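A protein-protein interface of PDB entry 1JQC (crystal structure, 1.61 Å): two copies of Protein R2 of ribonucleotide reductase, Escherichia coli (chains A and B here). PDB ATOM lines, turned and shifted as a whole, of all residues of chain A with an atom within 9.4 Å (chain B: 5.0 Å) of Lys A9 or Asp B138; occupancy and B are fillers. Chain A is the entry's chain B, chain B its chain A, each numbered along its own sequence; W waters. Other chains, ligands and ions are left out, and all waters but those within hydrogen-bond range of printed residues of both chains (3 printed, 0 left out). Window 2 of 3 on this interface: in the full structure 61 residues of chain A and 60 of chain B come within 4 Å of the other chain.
The side-chain hydroxyl of Ser B134 lies within hydrogen-bond range of the guanidinium group of Arg A27 (2.9 Å).
The backbone carbonyl oxygen (O) of Asp B138 is in hydrogen-bond range of the side-chain hydroxyl (OG1) of Thr B142 (3.4 Å).
O of Ser A6 lies within hydrogen-bond range of ND2 of Asn A24 (2.9 Å).
NE2 of Gln A21 lies within hydrogen-bond range of O of Thr A8 (2.9 Å).
The side-chain amide nitrogen (ND2) of Asn A24 is in hydrogen-bond range of the backbone carbonyl oxygen (O) of Thr A8, at 3.1 Å.
OE1 of Gln A12 sits close to O of Val A25 (3.0 Å).
The side-chain amide nitrogen (ND2) of Asn A24 sits close to the side-chain amide nitrogen (NE2) of Gln A21 (3.4 Å).
Among the printed residues, pairs that only touch across the chains: Gln A7 with Val B141 (3.6 Å), Thr A8 with Val B141 (3.8 Å), Lys A9 with Asp B138 (3.8 Å), Lys A9 with Val B141 (3.8 Å), Lys A9 with Thr B142 (3.6 Å), Asn A24 with Val B141 (3.7 Å), Val A25 with Phe B137 (3.7 Å), Val A25 with Ile B140 (3.95 Å), Val A25 with Val B141 (3.6 Å), Arg A27 with Phe B137 (3.4 Å), Asp A29 with Pro B133 (3.7 Å) and Asp A29 with Phe B137 (3.4 Å).
Of chain B, only Asp B138, Val B141 and Thr B142 come within 4 Å of Lys A9.
Of chain A, only Lys A9 comes within 4 Å of Asp B138.
Of chain A, only Gln A7, Thr A8, Lys A9, Asn A24 and Val A25 come within 4 Å of Val B141.
Printed residues of chain B within 4 Å of Thr A8: Val B141.
Of the printed residues of chain A, Thr B142 touches Lys A9 (3.6 Å).
Printed residues of chain B within 4 Å of Arg A27: Ser B134 and Phe B137.
Of the printed residues of chain B, Asp A29 touches Pro B133 and Phe B137.
Of the printed residues of chain B, Val A25 touches Phe B137, Ile B140 and Val B141.
Asp A11 touches none of the printed residues of chain B.
The nearest residue of chain A that does not touch Asp B138 is Arg A27 (4.2 Å).
Printed residues of chain B that touch a printed residue of chain A: Pro B133, Ser B134, Phe B137, Asp B138, Ile B140, Val B141 and Thr B142.
Among the printed residues, 13 pairs touch across the chains.
Among the printed residues, no Asp or Glu carboxylate lies within 4 Å of a Lys or Arg side-chain nitrogen of the other chain.
No position is printed for both chains.
Water W3 bridges OD1 of Asp B138 (2.5 Å) and O of Asn A10 (2.9 Å).
Water W1 lies within hydrogen-bond range of the side-chain carboxylate (OD2) of Asp B138 (3.0 Å), the guanidinium group (NH1) of Arg A27 (3.0 Å) and the side-chain hydroxyl (OG) of Ser B134 (3.4 Å).
Water W2 lies within hydrogen-bond range of NH1 of Arg A27 and OD1 of Asp B138.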
ATOM      1  N   PHE A   5      -9.033  -2.412  32.173  1.00  0.00           N
ATOM      2  CA  PHE A   5      -8.341  -3.327  31.239  1.00  0.00           C
ATOM      3  C   PHE A   5      -8.005  -2.570  29.938  1.00  0.00           C
ATOM      4  O   PHE A   5      -8.799  -2.450  29.018  1.00  0.00           O
ATOM      5  CB  PHE A   5      -9.147  -4.595  30.957  1.00  0.00           C
ATOM      6  CG  PHE A   5      -8.313  -5.691  30.342  1.00  0.00           C
ATOM      7  CD1 PHE A   5      -8.167  -5.804  28.961  1.00  0.00           C
ATOM      8  CD2 PHE A   5      -7.609  -6.563  31.166  1.00  0.00           C
ATOM      9  CE1 PHE A   5      -7.327  -6.792  28.408  1.00  0.00           C
ATOM     10  CE2 PHE A   5      -6.763  -7.559  30.638  1.00  0.00           C
ATOM     11  CZ  PHE A   5      -6.627  -7.672  29.219  1.00  0.00           C
ATOM     12  N   SER A   6      -6.784  -2.062  29.908  1.00  0.00           N
ATOM     13  CA  SER A   6      -6.298  -1.280  28.765  1.00  0.00           C
ATOM     14  C   SER A   6      -6.221  -2.222  27.565  1.00  0.00           C
ATOM     15  O   SER A   6      -5.562  -3.250  27.604  1.00  0.00           O
ATOM     16  CB  SER A   6      -4.949  -0.678  29.140  1.00  0.00           C
ATOM     17  OG  SER A   6      -4.029  -1.652  29.623  1.00  0.00           O
ATOM     18  N   GLN A   7      -6.871  -1.842  26.469  1.00  0.00           N
ATOM     19  CA  GLN A   7      -6.958  -2.759  25.338  1.00  0.00           C
ATOM     20  C   GLN A   7      -5.808  -2.685  24.339  1.00  0.00           C
ATOM     21  O   GLN A   7      -5.816  -3.365  23.316  1.00  0.00           O
ATOM     22  CB  GLN A   7      -8.334  -2.609  24.671  1.00  0.00           C
ATOM     23  CG  GLN A   7      -8.703  -1.176  24.349  1.00  0.00           C
ATOM     24  CD  GLN A   7     -10.193  -0.845  24.565  1.00  0.00           C
ATOM     25  OE1 GLN A   7     -10.575   0.328  24.550  1.00  0.00           O
ATOM     26  NE2 GLN A   7     -11.028  -1.869  24.755  1.00  0.00           N
ATOM     27  N   THR A   8      -4.808  -1.891  24.676  1.00  0.00           N
ATOM     28  CA  THR A   8      -3.601  -1.744  23.858  1.00  0.00           C
ATOM     29  C   THR A   8      -2.551  -2.790  24.278  1.00  0.00           C
ATOM     30  O   THR A   8      -2.193  -2.914  25.452  1.00  0.00           O
ATOM     31  CB  THR A   8      -3.023  -0.346  24.029  1.00  0.00           C
ATOM     32  OG1 THR A   8      -4.037   0.609  23.661  1.00  0.00           O
ATOM     33  CG2 THR A   8      -1.766  -0.166  23.170  1.00  0.00           C
ATOM     34  N   LYS A   9      -2.076  -3.579  23.325  1.00  0.00           N
ATOM     35  CA  LYS A   9      -1.060  -4.560  23.663  1.00  0.00           C
ATOM     36  C   LYS A   9       0.206  -3.712  23.911  1.00  0.00           C
ATOM     37  O   LYS A   9       0.599  -2.897  23.081  1.00  0.00           O
ATOM     38  CB  LYS A   9      -0.858  -5.507  22.471  1.00  0.00           C
ATOM     39  CG  LYS A   9       0.198  -6.534  22.681  1.00  0.00           C
ATOM     40  CD  LYS A   9       0.497  -7.174  21.333  1.00  0.00           C
ATOM     41  CE  LYS A   9       1.787  -7.938  21.376  1.00  0.00           C
ATOM     42  NZ  LYS A   9       2.222  -8.255  19.983  1.00  0.00           N
ATOM     43  N   ASN A  10       0.798  -3.852  25.086  1.00  0.00           N
ATOM     44  CA  ASN A  10       1.976  -3.094  25.438  1.00  0.00           C
ATOM     45  C   ASN A  10       3.037  -3.964  26.089  1.00  0.00           C
ATOM     46  O   ASN A  10       2.729  -4.993  26.692  1.00  0.00           O
ATOM     47  CB  ASN A  10       1.578  -1.911  26.364  1.00  0.00           C
ATOM     48  CG  ASN A  10       1.160  -2.343  27.788  1.00  0.00           C
ATOM     49  OD1 ASN A  10       0.377  -3.270  27.974  1.00  0.00           O
ATOM     50  ND2 ASN A  10       1.671  -1.621  28.780  1.00  0.00           N
ATOM     51  N   ASP A  11       4.279  -3.514  26.017  1.00  0.00           N
ATOM     52  CA  ASP A  11       5.385  -4.247  26.622  1.00  0.00           C
ATOM     53  C   ASP A  11       5.480  -3.769  28.064  1.00  0.00           C
ATOM     54  O   ASP A  11       5.969  -2.655  28.367  1.00  0.00           O
ATOM     55  CB  ASP A  11       6.702  -3.932  25.880  1.00  0.00           C
ATOM     56  CG  ASP A  11       7.871  -4.778  26.368  1.00  0.00           C
ATOM     57  OD1 ASP A  11       7.792  -5.366  27.470  1.00  0.00           O
ATOM     58  OD2 ASP A  11       8.908  -4.842  25.643  1.00  0.00           O
ATOM     59  N   GLN A  12       4.973  -4.600  28.969  1.00  0.00           N
ATOM     60  CA  GLN A  12       5.004  -4.258  30.392  1.00  0.00           C
ATOM     61  C   GLN A  12       6.398  -4.135  31.010  1.00  0.00           C
ATOM     62  O   GLN A  12       6.513  -3.618  32.105  1.00  0.00           O
ATOM     63  CB  GLN A  12       4.200  -5.304  31.196  1.00  0.00           C
ATOM     64  CG  GLN A  12       2.740  -5.359  30.781  1.00  0.00           C
ATOM     65  CD  GLN A  12       1.950  -6.404  31.515  1.00  0.00           C
ATOM     66  OE1 GLN A  12       0.726  -6.223  31.821  1.00  0.00           O
ATOM     67  NE2 GLN A  12       2.612  -7.493  31.838  1.00  0.00           N
ATOM     68  N   LEU A  13       7.469  -4.617  30.341  1.00  0.00           N
ATOM     69  CA  LEU A  13       8.792  -4.477  30.895  1.00  0.00           C
ATOM     70  C   LEU A  13       9.339  -3.059  30.617  1.00  0.00           C
ATOM     71  O   LEU A  13      10.332  -2.657  31.206  1.00  0.00           O
ATOM     72  CB  LEU A  13       9.752  -5.509  30.237  1.00  0.00           C
ATOM     73  CG  LEU A  13       9.432  -6.964  30.550  1.00  0.00           C
ATOM     74  CD1 LEU A  13      10.430  -7.866  29.765  1.00  0.00           C
ATOM     75  CD2 LEU A  13       9.518  -7.203  32.095  1.00  0.00           C
ATOM     76  N   GLU A  15       7.245  -0.188  30.574  1.00  0.00           N
ATOM     77  CA  GLU A  15       6.444   0.887  31.199  1.00  0.00           C
ATOM     78  C   GLU A  15       7.139   1.389  32.467  1.00  0.00           C
ATOM     79  O   GLU A  15       7.934   0.685  33.064  1.00  0.00           O
ATOM     80  CB  GLU A  15       5.090   0.309  31.676  1.00  0.00           C
ATOM     81  CG  GLU A  15       4.093  -0.132  30.607  1.00  0.00           C
ATOM     82  CD  GLU A  15       3.568   1.029  29.743  1.00  0.00           C
ATOM     83  OE1 GLU A  15       3.455   2.185  30.249  1.00  0.00           O
ATOM     84  OE2 GLU A  15       3.249   0.785  28.557  1.00  0.00           O
ATOM     85  N   GLN A  21       0.741   3.202  30.969  1.00  0.00           N
ATOM     86  CA  GLN A  21      -0.523   2.593  30.592  1.00  0.00           C
ATOM     87  C   GLN A  21      -1.022   1.724  31.778  1.00  0.00           C
ATOM     88  O   GLN A  21      -0.243   0.991  32.374  1.00  0.00           O
ATOM     89  CB  GLN A  21      -0.327   1.669  29.381  1.00  0.00           C
ATOM     90  CG  GLN A  21      -1.625   1.023  28.943  1.00  0.00           C
ATOM     91  CD  GLN A  21      -1.428   0.149  27.707  1.00  0.00           C
ATOM     92  OE1 GLN A  21      -0.760   0.555  26.764  1.00  0.00           O
ATOM     93  NE2 GLN A  21      -2.000  -1.036  27.715  1.00  0.00           N
ATOM     94  N   PRO A  22      -2.314   1.820  32.125  1.00  0.00           N
ATOM     95  CA  PRO A  22      -2.827   0.997  33.228  1.00  0.00           C
ATOM     96  C   PRO A  22      -2.553  -0.473  32.917  1.00  0.00           C
ATOM     97  O   PRO A  22      -2.581  -0.861  31.756  1.00  0.00           O
ATOM     98  CB  PRO A  22      -4.329   1.345  33.240  1.00  0.00           C
ATOM     99  CG  PRO A  22      -4.286   2.819  32.887  1.00  0.00           C
ATOM    100  CD  PRO A  22      -3.311   2.835  31.707  1.00  0.00           C
ATOM    101  N   ASN A  24      -2.957  -4.235  32.086  1.00  0.00           N
ATOM    102  CA  ASN A  24      -4.039  -5.038  31.549  1.00  0.00           C
ATOM    103  C   ASN A  24      -3.883  -6.466  32.098  1.00  0.00           C
ATOM    104  O   ASN A  24      -4.527  -6.811  33.097  1.00  0.00           O
ATOM    105  CB  ASN A  24      -4.186  -5.001  29.991  1.00  0.00           C
ATOM    106  CG  ASN A  24      -2.891  -5.063  29.196  1.00  0.00           C
ATOM    107  OD1 ASN A  24      -1.951  -5.805  29.507  1.00  0.00           O
ATOM    108  ND2 ASN A  24      -2.878  -4.326  28.089  1.00  0.00           N
ATOM    109  N   VAL A  25      -3.046  -7.308  31.504  1.00  0.00           N
ATOM    110  CA  VAL A  25      -2.906  -8.666  32.026  1.00  0.00           C
ATOM    111  C   VAL A  25      -2.003  -8.787  33.259  1.00  0.00           C
ATOM    112  O   VAL A  25      -0.911  -8.242  33.350  1.00  0.00           O
ATOM    113  CB  VAL A  25      -2.293  -9.563  30.927  1.00  0.00           C
ATOM    114  CG1 VAL A  25      -1.958 -10.969  31.482  1.00  0.00           C
ATOM    115  CG2 VAL A  25      -3.221  -9.620  29.773  1.00  0.00           C
ATOM    116  N   ARG A  27       0.375 -10.920  34.943  1.00  0.00           N
ATOM    117  CA  ARG A  27       1.284 -12.076  34.706  1.00  0.00           C
ATOM    118  C   ARG A  27       2.496 -11.905  35.625  1.00  0.00           C
ATOM    119  O   ARG A  27       2.920 -10.774  35.933  1.00  0.00           O
ATOM    120  CB  ARG A  27       1.742 -12.102  33.246  1.00  0.00           C
ATOM    121  CG  ARG A  27       2.464 -10.829  32.804  1.00  0.00           C
ATOM    122  CD  ARG A  27       2.757 -10.740  31.259  1.00  0.00           C
ATOM    123  NE  ARG A  27       3.749 -11.722  30.869  1.00  0.00           N
ATOM    124  CZ  ARG A  27       4.260 -11.818  29.647  1.00  0.00           C
ATOM    125  NH1 ARG A  27       3.856 -11.011  28.697  1.00  0.00           N
ATOM    126  NH2 ARG A  27       5.221 -12.695  29.421  1.00  0.00           N
ATOM    127  N   ASP A  29       5.512 -14.079  35.209  1.00  0.00           N
ATOM    128  CA  ASP A  29       6.613 -14.887  34.653  1.00  0.00           C
ATOM    129  C   ASP A  29       7.803 -14.033  34.302  1.00  0.00           C
ATOM    130  O   ASP A  29       8.869 -14.560  33.954  1.00  0.00           O
ATOM    131  CB  ASP A  29       6.131 -15.584  33.398  1.00  0.00           C
ATOM    132  CG  ASP A  29       5.667 -14.605  32.350  1.00  0.00           C
ATOM    133  OD1 ASP A  29       4.796 -13.754  32.621  1.00  0.00           O
ATOM    134  OD2 ASP A  29       6.142 -14.656  31.201  1.00  0.00           O
ATOM    135  N   GLN A  30       7.638 -12.712  34.362  1.00  0.00           N
ATOM    136  CA  GLN A  30       8.724 -11.805  34.040  1.00  0.00           C
ATOM    137  C   GLN A  30       8.407 -10.506  34.749  1.00  0.00           C
ATOM    138  O   GLN A  30       7.266 -10.250  35.108  1.00  0.00           O
ATOM    139  CB  GLN A  30       8.793 -11.509  32.527  1.00  0.00           C
ATOM    140  CG  GLN A  30       7.446 -11.067  31.929  1.00  0.00           C
ATOM    141  CD  GLN A  30       7.508 -10.478  30.521  1.00  0.00           C
ATOM    142  OE1 GLN A  30       6.735  -9.573  30.181  1.00  0.00           O
ATOM    143  NE2 GLN A  30       8.404 -11.007  29.689  1.00  0.00           N
ATOM    144  N   PRO B 133       5.468 -18.189  27.354  1.00  0.00           N
ATOM    145  CA  PRO B 133       4.243 -17.685  27.993  1.00  0.00           C
ATOM    146  C   PRO B 133       3.786 -16.403  27.381  1.00  0.00           C
ATOM    147  O   PRO B 133       2.600 -16.131  27.367  1.00  0.00           O
ATOM    148  CB  PRO B 133       4.664 -17.503  29.442  1.00  0.00           C
ATOM    149  CG  PRO B 133       5.681 -18.592  29.623  1.00  0.00           C
ATOM    150  CD  PRO B 133       6.503 -18.472  28.367  1.00  0.00           C
ATOM    151  N   SER B 134       4.715 -15.601  26.868  1.00  0.00           N
ATOM    152  CA  SER B 134       4.329 -14.322  26.283  1.00  0.00           C
ATOM    153  C   SER B 134       3.322 -14.453  25.163  1.00  0.00           C
ATOM    154  O   SER B 134       2.465 -13.602  24.989  1.00  0.00           O
ATOM    155  CB  SER B 134       5.554 -13.584  25.746  1.00  0.00           C
ATOM    156  OG  SER B 134       6.369 -13.107  26.809  1.00  0.00           O
ATOM    157  N   VAL B 135       3.415 -15.504  24.369  1.00  0.00           N
ATOM    158  CA  VAL B 135       2.462 -15.569  23.266  1.00  0.00           C
ATOM    159  C   VAL B 135       1.061 -15.736  23.798  1.00  0.00           C
ATOM    160  O   VAL B 135       0.130 -15.164  23.243  1.00  0.00           O
ATOM    161  CB  VAL B 135       2.818 -16.688  22.269  1.00  0.00           C
ATOM    162  CG1 VAL B 135       1.613 -16.971  21.341  1.00  0.00           C
ATOM    163  CG2 VAL B 135       4.007 -16.232  21.438  1.00  0.00           C
ATOM    164  N   VAL B 136       0.928 -16.485  24.892  1.00  0.00           N
ATOM    165  CA  VAL B 136      -0.368 -16.718  25.524  1.00  0.00           C
ATOM    166  C   VAL B 136      -0.859 -15.383  26.139  1.00  0.00           C
ATOM    167  O   VAL B 136      -1.944 -14.895  25.816  1.00  0.00           O
ATOM    168  CB  VAL B 136      -0.246 -17.848  26.630  1.00  0.00           C
ATOM    169  CG1 VAL B 136      -1.624 -18.050  27.353  1.00  0.00           C
ATOM    170  CG2 VAL B 136       0.154 -19.186  25.971  1.00  0.00           C
ATOM    171  N   PHE B 137      -0.030 -14.770  26.981  1.00  0.00           N
ATOM    172  CA  PHE B 137      -0.418 -13.499  27.613  1.00  0.00           C
ATOM    173  C   PHE B 137      -0.703 -12.379  26.643  1.00  0.00           C
ATOM    174  O   PHE B 137      -1.705 -11.640  26.799  1.00  0.00           O
ATOM    175  CB  PHE B 137       0.652 -13.061  28.645  1.00  0.00           C
ATOM    176  CG  PHE B 137       0.755 -13.986  29.861  1.00  0.00           C
ATOM    177  CD1 PHE B 137      -0.369 -14.257  30.647  1.00  0.00           C
ATOM    178  CD2 PHE B 137       1.986 -14.546  30.234  1.00  0.00           C
ATOM    179  CE1 PHE B 137      -0.250 -15.067  31.788  1.00  0.00           C
ATOM    180  CE2 PHE B 137       2.112 -15.353  31.359  1.00  0.00           C
ATOM    181  CZ  PHE B 137       0.991 -15.620  32.147  1.00  0.00           C
ATOM    182  N   ASP B 138       0.114 -12.220  25.609  1.00  0.00           N
ATOM    183  CA  ASP B 138      -0.186 -11.134  24.661  1.00  0.00           C
ATOM    184  C   ASP B 138      -1.491 -11.357  23.908  1.00  0.00           C
ATOM    185  O   ASP B 138      -2.233 -10.397  23.603  1.00  0.00           O
ATOM    186  CB  ASP B 138       0.939 -10.971  23.633  1.00  0.00           C
ATOM    187  CG  ASP B 138       2.183 -10.348  24.224  1.00  0.00           C
ATOM    188  OD1 ASP B 138       2.074  -9.564  25.200  1.00  0.00           O
ATOM    189  OD2 ASP B 138       3.275 -10.635  23.692  1.00  0.00           O
ATOM    190  N   ASP B 139      -1.794 -12.618  23.613  1.00  0.00           N
ATOM    191  CA  ASP B 139      -3.030 -12.909  22.893  1.00  0.00           C
ATOM    192  C   ASP B 139      -4.299 -12.549  23.675  1.00  0.00           C
ATOM    193  O   ASP B 139      -5.371 -12.279  23.110  1.00  0.00           O
ATOM    194  CB  ASP B 139      -3.058 -14.392  22.463  1.00  0.00           C
ATOM    195  CG  ASP B 139      -4.212 -14.680  21.513  1.00  0.00           C
ATOM    196  OD1 ASP B 139      -4.306 -14.001  20.474  1.00  0.00           O
ATOM    197  OD2 ASP B 139      -5.037 -15.545  21.814  1.00  0.00           O
ATOM    198  N   ILE B 140      -4.186 -12.536  24.994  1.00  0.00           N
ATOM    199  CA  ILE B 140      -5.349 -12.217  25.809  1.00  0.00           C
ATOM    200  C   ILE B 140      -5.814 -10.806  25.486  1.00  0.00           C
ATOM    201  O   ILE B 140      -7.011 -10.543  25.304  1.00  0.00           O
ATOM    202  CB  ILE B 140      -4.992 -12.320  27.294  1.00  0.00           C
ATOM    203  CG1 ILE B 140      -4.758 -13.794  27.657  1.00  0.00           C
ATOM    204  CG2 ILE B 140      -6.150 -11.714  28.143  1.00  0.00           C
ATOM    205  CD1 ILE B 140      -4.208 -14.015  28.995  1.00  0.00           C
ATOM    206  N   VAL B 141      -4.857  -9.896  25.375  1.00  0.00           N
ATOM    207  CA  VAL B 141      -5.188  -8.514  25.085  1.00  0.00           C
ATOM    208  C   VAL B 141      -5.763  -8.278  23.700  1.00  0.00           C
ATOM    209  O   VAL B 141      -6.765  -7.587  23.538  1.00  0.00           O
ATOM    210  CB  VAL B 141      -3.925  -7.609  25.243  1.00  0.00           C
ATOM    211  CG1 VAL B 141      -4.289  -6.133  25.028  1.00  0.00           C
ATOM    212  CG2 VAL B 141      -3.332  -7.779  26.644  1.00  0.00           C
ATOM    213  N   THR B 142      -5.122  -8.881  22.711  1.00  0.00           N
ATOM    214  CA  THR B 142      -5.475  -8.695  21.307  1.00  0.00           C
ATOM    215  C   THR B 142      -6.494  -9.652  20.706  1.00  0.00           C
ATOM    216  O   THR B 142      -6.990  -9.416  19.607  1.00  0.00           O
ATOM    217  CB  THR B 142      -4.179  -8.756  20.430  1.00  0.00           C
ATOM    218  OG1 THR B 142      -3.601 -10.069  20.471  1.00  0.00           O
ATOM    219  CG2 THR B 142      -3.142  -7.769  20.949  1.00  0.00           C
HETATM  220  O   HOH W   1       4.933 -10.089  26.080  1.00  0.00           O
HETATM  221  O   HOH W   2       1.828  -8.799  28.211  1.00  0.00           O
HETATM  222  O   HOH W   3       3.356  -7.369  25.129  1.00  0.00           O
